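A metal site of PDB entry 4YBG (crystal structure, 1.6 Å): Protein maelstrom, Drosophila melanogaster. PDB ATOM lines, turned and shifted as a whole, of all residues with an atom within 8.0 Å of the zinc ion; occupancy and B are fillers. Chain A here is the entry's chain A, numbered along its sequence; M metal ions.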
ATOM      1  N   ASN A  38     -11.869  -6.846   5.910  1.00  0.00           N
ATOM      2  CA  ASN A  38     -13.229  -7.379   5.786  1.00  0.00           C
ATOM      3  C   ASN A  38     -13.701  -7.198   4.371  1.00  0.00           C
ATOM      4  O   ASN A  38     -13.243  -6.265   3.689  1.00  0.00           O
ATOM      5  CB  ASN A  38     -14.214  -6.695   6.726  1.00  0.00           C
ATOM      6  CG  ASN A  38     -14.290  -7.384   8.087  1.00  0.00           C
ATOM      7  OD1 ASN A  38     -14.441  -8.635   8.163  1.00  0.00           O
ATOM      8  ND2 ASN A  38     -14.179  -6.607   9.177  1.00  0.00           N
ATOM      9  N   ALA A  52     -14.490  -3.933   2.642  1.00  0.00           N
ATOM     10  CA  ALA A  52     -15.372  -3.254   3.592  1.00  0.00           C
ATOM     11  C   ALA A  52     -14.633  -2.591   4.742  1.00  0.00           C
ATOM     12  O   ALA A  52     -15.149  -1.651   5.363  1.00  0.00           O
ATOM     13  CB  ALA A  52     -16.378  -4.238   4.186  1.00  0.00           C
ATOM     14  N   GLU A  53     -13.469  -3.118   5.102  1.00  0.00           N
ATOM     15  CA  GLU A  53     -12.746  -2.614   6.257  1.00  0.00           C
ATOM     16  C   GLU A  53     -11.300  -3.026   6.136  1.00  0.00           C
ATOM     17  O   GLU A  53     -11.051  -4.093   5.574  1.00  0.00           O
ATOM     18  CB  GLU A  53     -13.313  -3.176   7.578  1.00  0.00           C
ATOM     19  CG  GLU A  53     -13.018  -2.262   8.794  1.00  0.00           C
ATOM     20  CD  GLU A  53     -13.509  -2.823  10.102  1.00  0.00           C
ATOM     21  OE1 GLU A  53     -13.819  -4.029  10.207  1.00  0.00           O
ATOM     22  OE2 GLU A  53     -13.652  -2.003  11.052  1.00  0.00           O
ATOM     23  N   PHE A  54     -10.372  -2.221   6.650  1.00  0.00           N
ATOM     24  CA  PHE A  54      -8.951  -2.611   6.595  1.00  0.00           C
ATOM     25  C   PHE A  54      -8.257  -2.163   7.860  1.00  0.00           C
ATOM     26  O   PHE A  54      -8.499  -1.058   8.346  1.00  0.00           O
ATOM     27  CB  PHE A  54      -8.265  -1.968   5.393  1.00  0.00           C
ATOM     28  CG  PHE A  54      -6.765  -2.180   5.380  1.00  0.00           C
ATOM     29  CD1 PHE A  54      -6.240  -3.360   4.867  1.00  0.00           C
ATOM     30  CD2 PHE A  54      -5.882  -1.189   5.829  1.00  0.00           C
ATOM     31  CE1 PHE A  54      -4.856  -3.573   4.787  1.00  0.00           C
ATOM     32  CE2 PHE A  54      -4.496  -1.381   5.759  1.00  0.00           C
ATOM     33  CZ  PHE A  54      -3.977  -2.594   5.254  1.00  0.00           C
ATOM     34  N   ALA A  55      -7.346  -3.000   8.380  1.00  0.00           N
ATOM     35  CA  ALA A  55      -6.425  -2.481   9.395  1.00  0.00           C
ATOM     36  C   ALA A  55      -5.087  -3.072   9.159  1.00  0.00           C
ATOM     37  O   ALA A  55      -4.967  -4.149   8.576  1.00  0.00           O
ATOM     38  CB  ALA A  55      -6.919  -2.806  10.836  1.00  0.00           C
ATOM     39  N   SER A  70      -6.178   2.094  10.469  1.00  0.00           N
ATOM     40  CA  SER A  70      -7.496   1.479  10.500  1.00  0.00           C
ATOM     41  C   SER A  70      -8.540   2.351   9.808  1.00  0.00           C
ATOM     42  O   SER A  70      -8.615   3.551  10.087  1.00  0.00           O
ATOM     43  CB  SER A  70      -7.911   1.226  11.952  1.00  0.00           C
ATOM     44  OG  SER A  70      -9.279   0.873  12.088  1.00  0.00           O
ATOM     45  N   THR A  71      -9.316   1.753   8.904  1.00  0.00           N
ATOM     46  CA  THR A  71     -10.354   2.508   8.185  1.00  0.00           C
ATOM     47  C   THR A  71     -11.498   1.605   7.716  1.00  0.00           C
ATOM     48  O   THR A  71     -11.280   0.462   7.372  1.00  0.00           O
ATOM     49  CB  THR A  71      -9.770   3.236   7.003  1.00  0.00           C
ATOM     50  OG1 THR A  71     -10.759   4.144   6.463  1.00  0.00           O
ATOM     51  CG2 THR A  71      -9.323   2.267   5.920  1.00  0.00           C
ATOM     52  N   MET A  72     -12.722   2.119   7.769  1.00  0.00           N
ATOM     53  CA  MET A  72     -13.818   1.466   7.037  1.00  0.00           C
ATOM     54  C   MET A  72     -13.693   1.872   5.562  1.00  0.00           C
ATOM     55  O   MET A  72     -13.058   2.904   5.199  1.00  0.00           O
ATOM     56  CB  MET A  72     -15.189   1.849   7.635  1.00  0.00           C
ATOM     57  CG  MET A  72     -15.505   1.049   8.972  1.00  0.00           C
ATOM     58  SD  MET A  72     -16.925   1.811   9.864  1.00  0.00           S
ATOM     59  CE  MET A  72     -16.492   3.539   9.892  1.00  0.00           C
ATOM     60  N   HIS A  94     -18.955  -9.014  10.243  1.00  0.00           N
ATOM     61  CA  HIS A  94     -18.720  -7.623  10.622  1.00  0.00           C
ATOM     62  C   HIS A  94     -19.962  -6.730  10.735  1.00  0.00           C
ATOM     63  O   HIS A  94     -19.955  -5.712  11.444  1.00  0.00           O
ATOM     64  CB  HIS A  94     -17.717  -7.002   9.620  1.00  0.00           C
ATOM     65  CG  HIS A  94     -18.113  -7.148   8.175  1.00  0.00           C
ATOM     66  ND1 HIS A  94     -19.106  -6.362   7.610  1.00  0.00           N
ATOM     67  CD2 HIS A  94     -17.647  -7.940   7.177  1.00  0.00           C
ATOM     68  CE1 HIS A  94     -19.256  -6.699   6.336  1.00  0.00           C
ATOM     69  NE2 HIS A  94     -18.367  -7.632   6.040  1.00  0.00           N
ATOM     70  N   LEU A  96     -21.141  -4.517   8.901  1.00  0.00           N
ATOM     71  CA  LEU A  96     -21.059  -3.148   8.368  1.00  0.00           C
ATOM     72  C   LEU A  96     -22.201  -2.911   7.406  1.00  0.00           C
ATOM     73  O   LEU A  96     -22.590  -3.820   6.670  1.00  0.00           O
ATOM     74  CB  LEU A  96     -19.714  -2.924   7.681  1.00  0.00           C
ATOM     75  CG  LEU A  96     -18.497  -2.939   8.615  1.00  0.00           C
ATOM     76  CD1 LEU A  96     -17.202  -3.274   7.915  1.00  0.00           C
ATOM     77  CD2 LEU A  96     -18.414  -1.560   9.273  1.00  0.00           C
ATOM     78  N   ILE A 208     -10.539  -2.346  21.837  1.00  0.00           N
ATOM     79  CA  ILE A 208      -9.547  -2.458  20.767  1.00  0.00           C
ATOM     80  C   ILE A 208     -10.182  -2.453  19.375  1.00  0.00           C
ATOM     81  O   ILE A 208      -9.470  -2.410  18.384  1.00  0.00           O
ATOM     82  CB  ILE A 208      -8.632  -3.709  20.943  1.00  0.00           C
ATOM     83  CG1 ILE A 208      -9.448  -5.002  20.985  1.00  0.00           C
ATOM     84  CG2 ILE A 208      -7.756  -3.544  22.213  1.00  0.00           C
ATOM     85  CD1 ILE A 208      -8.596  -6.325  20.887  1.00  0.00           C
ATOM     86  N   ALA A 209     -11.505  -2.485  19.308  1.00  0.00           N
ATOM     87  CA  ALA A 209     -12.173  -2.380  18.014  1.00  0.00           C
ATOM     88  C   ALA A 209     -12.344  -0.932  17.596  1.00  0.00           C
ATOM     89  O   ALA A 209     -12.140   0.006  18.373  1.00  0.00           O
ATOM     90  CB  ALA A 209     -13.524  -3.069  18.042  1.00  0.00           C
ATOM     91  N   CYS A 210     -12.786  -0.753  16.357  1.00  0.00           N
ATOM     92  CA  CYS A 210     -13.130   0.604  15.904  1.00  0.00           C
ATOM     93  C   CYS A 210     -14.418   1.017  16.583  1.00  0.00           C
ATOM     94  O   CYS A 210     -15.082   0.210  17.200  1.00  0.00           O
ATOM     95  CB  CYS A 210     -13.277   0.618  14.376  1.00  0.00           C
ATOM     96  SG  CYS A 210     -14.758  -0.218  13.702  1.00  0.00           S
ATOM     97  N   GLN A 211     -14.798   2.290  16.473  1.00  0.00           N
ATOM     98  CA  GLN A 211     -15.980   2.771  17.187  1.00  0.00           C
ATOM     99  C   GLN A 211     -17.260   2.094  16.693  1.00  0.00           C
ATOM    100  O   GLN A 211     -18.137   1.761  17.495  1.00  0.00           O
ATOM    101  CB  GLN A 211     -16.098   4.284  17.031  1.00  0.00           C
ATOM    102  CG  GLN A 211     -17.273   4.923  17.754  1.00  0.00           C
ATOM    103  CD  GLN A 211     -17.309   4.625  19.267  1.00  0.00           C
ATOM    104  OE1 GLN A 211     -16.261   4.554  19.935  1.00  0.00           O
ATOM    105  NE2 GLN A 211     -18.510   4.458  19.794  1.00  0.00           N
ATOM    106  N   TYR A 212     -17.379   1.901  15.389  1.00  0.00           N
ATOM    107  CA  TYR A 212     -18.583   1.252  14.896  1.00  0.00           C
ATOM    108  C   TYR A 212     -18.736  -0.138  15.499  1.00  0.00           C
ATOM    109  O   TYR A 212     -19.861  -0.590  15.854  1.00  0.00           O
ATOM    110  CB  TYR A 212     -18.592   1.130  13.369  1.00  0.00           C
ATOM    111  CG  TYR A 212     -19.792   0.368  12.862  1.00  0.00           C
ATOM    112  CD1 TYR A 212     -21.023   1.000  12.708  1.00  0.00           C
ATOM    113  CD2 TYR A 212     -19.702  -0.991  12.567  1.00  0.00           C
ATOM    114  CE1 TYR A 212     -22.154   0.292  12.254  1.00  0.00           C
ATOM    115  CE2 TYR A 212     -20.796  -1.703  12.122  1.00  0.00           C
ATOM    116  CZ  TYR A 212     -22.010  -1.067  11.952  1.00  0.00           C
ATOM    117  OH  TYR A 212     -23.080  -1.812  11.493  1.00  0.00           O
ATOM    118  N   HIS A 213     -17.628  -0.864  15.552  1.00  0.00           N
ATOM    119  CA  HIS A 213     -17.706  -2.238  15.998  1.00  0.00           C
ATOM    120  C   HIS A 213     -17.831  -2.339  17.501  1.00  0.00           C
ATOM    121  O   HIS A 213     -18.431  -3.298  17.984  1.00  0.00           O
ATOM    122  CB  HIS A 213     -16.529  -3.038  15.450  1.00  0.00           C
ATOM    123  CG  HIS A 213     -16.802  -3.522  14.060  1.00  0.00           C
ATOM    124  ND1 HIS A 213     -15.946  -3.302  12.995  1.00  0.00           N
ATOM    125  CD2 HIS A 213     -17.897  -4.125  13.542  1.00  0.00           C
ATOM    126  CE1 HIS A 213     -16.487  -3.809  11.894  1.00  0.00           C
ATOM    127  NE2 HIS A 213     -17.665  -4.325  12.200  1.00  0.00           N
ATOM    128  N   GLU A 214     -17.390  -1.328  18.226  1.00  0.00           N
ATOM    129  CA  GLU A 214     -17.825  -1.252  19.620  1.00  0.00           C
ATOM    130  C   GLU A 214     -19.341  -0.989  19.699  1.00  0.00           C
ATOM    131  O   GLU A 214     -20.058  -1.582  20.514  1.00  0.00           O
ATOM    132  CB  GLU A 214     -17.034  -0.163  20.349  1.00  0.00           C
ATOM    133  CG  GLU A 214     -15.517  -0.467  20.412  1.00  0.00           C
ATOM    134  CD  GLU A 214     -15.182  -1.587  21.366  1.00  0.00           C
ATOM    135  OE1 GLU A 214     -16.059  -1.910  22.210  1.00  0.00           O
ATOM    136  OE2 GLU A 214     -14.076  -2.165  21.285  1.00  0.00           O
ATOM    137  N   ASN A 216     -21.773  -1.854  17.617  1.00  0.00           N
ATOM    138  CA  ASN A 216     -22.662  -2.931  17.161  1.00  0.00           C
ATOM    139  C   ASN A 216     -22.245  -4.301  17.736  1.00  0.00           C
ATOM    140  O   ASN A 216     -22.845  -5.331  17.396  1.00  0.00           O
ATOM    141  CB  ASN A 216     -22.736  -2.933  15.624  1.00  0.00           C
ATOM    142  CG  ASN A 216     -21.654  -3.774  14.946  1.00  0.00           C
ATOM    143  OD1 ASN A 216     -20.582  -4.021  15.516  1.00  0.00           O
ATOM    144  ND2 ASN A 216     -21.933  -4.230  13.725  1.00  0.00           N
ATOM    145  N   ARG A 218     -19.794  -6.269  17.252  1.00  0.00           N
ATOM    146  CA  ARG A 218     -19.181  -7.280  16.409  1.00  0.00           C
ATOM    147  C   ARG A 218     -17.660  -7.134  16.432  1.00  0.00           C
ATOM    148  O   ARG A 218     -16.983  -7.245  15.409  1.00  0.00           O
ATOM    149  CB  ARG A 218     -19.726  -7.185  14.986  1.00  0.00           C
ATOM    150  CG  ARG A 218     -21.210  -7.498  14.817  1.00  0.00           C
ATOM    151  CD  ARG A 218     -21.584  -8.913  15.212  1.00  0.00           C
ATOM    152  NE  ARG A 218     -23.018  -9.138  15.049  1.00  0.00           N
ATOM    153  CZ  ARG A 218     -23.582  -9.574  13.922  1.00  0.00           C
ATOM    154  NH1 ARG A 218     -24.891  -9.762  13.853  1.00  0.00           N
ATOM    155  NH2 ARG A 218     -22.812  -9.828  12.865  1.00  0.00           N
ATOM    156  N   THR A 219     -17.091  -6.944  17.618  1.00  0.00           N
ATOM    157  CA  THR A 219     -15.642  -6.717  17.707  1.00  0.00           C
ATOM    158  C   THR A 219     -14.823  -7.930  17.243  1.00  0.00           C
ATOM    159  O   THR A 219     -13.669  -7.793  16.774  1.00  0.00           O
ATOM    160  CB  THR A 219     -15.225  -6.277  19.132  1.00  0.00           C
ATOM    161  OG1 THR A 219     -15.740  -4.958  19.396  1.00  0.00           O
ATOM    162  CG2 THR A 219     -13.708  -6.279  19.327  1.00  0.00           C
ATOM    163  N   TYR A 221     -15.130  -9.539  14.653  1.00  0.00           N
ATOM    164  CA  TYR A 221     -14.975  -9.395  13.196  1.00  0.00           C
ATOM    165  C   TYR A 221     -14.590  -8.008  12.795  1.00  0.00           C
ATOM    166  O   TYR A 221     -14.893  -7.594  11.678  1.00  0.00           O
ATOM    167  CB  TYR A 221     -16.290  -9.795  12.504  1.00  0.00           C
ATOM    168  CG  TYR A 221     -16.625 -11.251  12.771  1.00  0.00           C
ATOM    169  CD1 TYR A 221     -15.860 -12.264  12.216  1.00  0.00           C
ATOM    170  CD2 TYR A 221     -17.657 -11.597  13.619  1.00  0.00           C
ATOM    171  CE1 TYR A 221     -16.143 -13.597  12.458  1.00  0.00           C
ATOM    172  CE2 TYR A 221     -17.955 -12.942  13.871  1.00  0.00           C
ATOM    173  CZ  TYR A 221     -17.174 -13.926  13.279  1.00  0.00           C
ATOM    174  OH  TYR A 221     -17.436 -15.259  13.515  1.00  0.00           O
ATOM    175  N   CYS A 222     -13.903  -7.290  13.673  1.00  0.00           N
ATOM    176  CA  CYS A 222     -13.434  -5.931  13.324  1.00  0.00           C
ATOM    177  C   CYS A 222     -11.979  -6.011  12.924  1.00  0.00           C
ATOM    178  O   CYS A 222     -11.213  -6.617  13.658  1.00  0.00           O
ATOM    179  CB  CYS A 222     -13.604  -4.988  14.534  1.00  0.00           C
ATOM    180  SG  CYS A 222     -12.707  -3.396  14.326  1.00  0.00           S
ATOM    181  N   THR A 223     -11.568  -5.450  11.784  1.00  0.00           N
ATOM    182  CA  THR A 223     -10.170  -5.603  11.366  1.00  0.00           C
ATOM    183  C   THR A 223      -9.209  -4.981  12.362  1.00  0.00           C
ATOM    184  O   THR A 223      -8.106  -5.507  12.566  1.00  0.00           O
ATOM    185  CB  THR A 223      -9.928  -4.993   9.992  1.00  0.00           C
ATOM    186  OG1 THR A 223     -10.480  -3.691   9.931  1.00  0.00           O
ATOM    187  CG2 THR A 223     -10.592  -5.863   8.898  1.00  0.00           C
ATOM    188  N   GLN A 224      -9.595  -3.888  12.995  1.00  0.00           N
ATOM    189  CA  GLN A 224      -8.701  -3.202  13.928  1.00  0.00           C
ATOM    190  C   GLN A 224      -8.524  -4.073  15.158  1.00  0.00           C
ATOM    191  O   GLN A 224      -7.420  -4.233  15.668  1.00  0.00           O
ATOM    192  CB  GLN A 224      -9.286  -1.842  14.319  1.00  0.00           C
ATOM    193  CG  GLN A 224      -8.353  -0.966  15.173  1.00  0.00           C
ATOM    194  CD  GLN A 224      -9.024   0.300  15.603  1.00  0.00           C
ATOM    195  OE1 GLN A 224      -9.512   1.081  14.796  1.00  0.00           O
ATOM    196  NE2 GLN A 224      -9.068   0.515  16.914  1.00  0.00           N
ATOM    197  N   SER A 225      -9.615  -4.675  15.612  1.00  0.00           N
ATOM    198  CA  SER A 225      -9.498  -5.608  16.748  1.00  0.00           C
ATOM    199  C   SER A 225      -8.631  -6.835  16.354  1.00  0.00           C
ATOM    200  O   SER A 225      -7.759  -7.255  17.113  1.00  0.00           O
ATOM    201  CB  SER A 225     -10.868  -6.084  17.173  1.00  0.00           C
ATOM    202  OG  SER A 225     -10.722  -7.079  18.208  1.00  0.00           O
ATOM    203  N   MET A 226      -8.875  -7.387  15.166  1.00  0.00           N
ATOM    204  CA  MET A 226      -8.152  -8.589  14.763  1.00  0.00           C
ATOM    205  C   MET A 226      -6.618  -8.384  14.742  1.00  0.00           C
ATOM    206  O   MET A 226      -5.901  -9.210  15.344  1.00  0.00           O
ATOM    207  CB  MET A 226      -8.698  -9.096  13.406  1.00  0.00           C
ATOM    208  CG  MET A 226     -10.133  -9.652  13.507  1.00  0.00           C
ATOM    209  SD  MET A 226     -10.904  -9.841  11.872  1.00  0.00           S
ATOM    210  CE  MET A 226      -9.597 -10.721  11.076  1.00  0.00           C
HETATM  211 ZN    ZN M   1     -14.188  -2.269  12.961  1.00  0.00          ZN
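Within 4 Å of the zinc ion: Glu 53, Cys 210, His 213 and Cys 222.
The nearest printed residue that does not touch the zinc ion is Thr 223 (4.3 Å).
SG of Cys 210 lies close to N of Tyr 212 (3.8 Å).
The side-chain carboxylate of Glu 53 lies within hydrogen-bond range of the side-chain amide nitrogen of Asn 38 (2.8 Å).
OG1 of Thr 219 is in hydrogen-bond range of O of His 213 (3.5 Å).
The side-chain sulfur (SG) of Cys 222 sits close to the backbone NH (N) of Ser 225, at 3.6 Å.
O of His 213 lies close to OD1 of Asn 216, at 3.4 Å.
The side-chain sulfur (SG) of Cys 222 lies close to the backbone NH (N) of Gln 224 (3.4 Å).
The backbone carbonyl oxygen (O) of His 213 sits at hydrogen-bond distance from the backbone NH (N) of Arg 218 (3.3 Å).
A ring nitrogen (NE2) of His 213 lies within hydrogen-bond range of the backbone carbonyl oxygen (O) of His 94 (2.8 Å).
The zinc ion is bound by the side-chain carboxylate (OE2) of Glu 53 (2.0 Å), a ring nitrogen (ND1) of His 213 (2.0 Å), the side-chain sulfur (SG) of Cys 210 (2.3 Å) and the side-chain sulfur (SG) of Cys 222 (2.3 Å).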
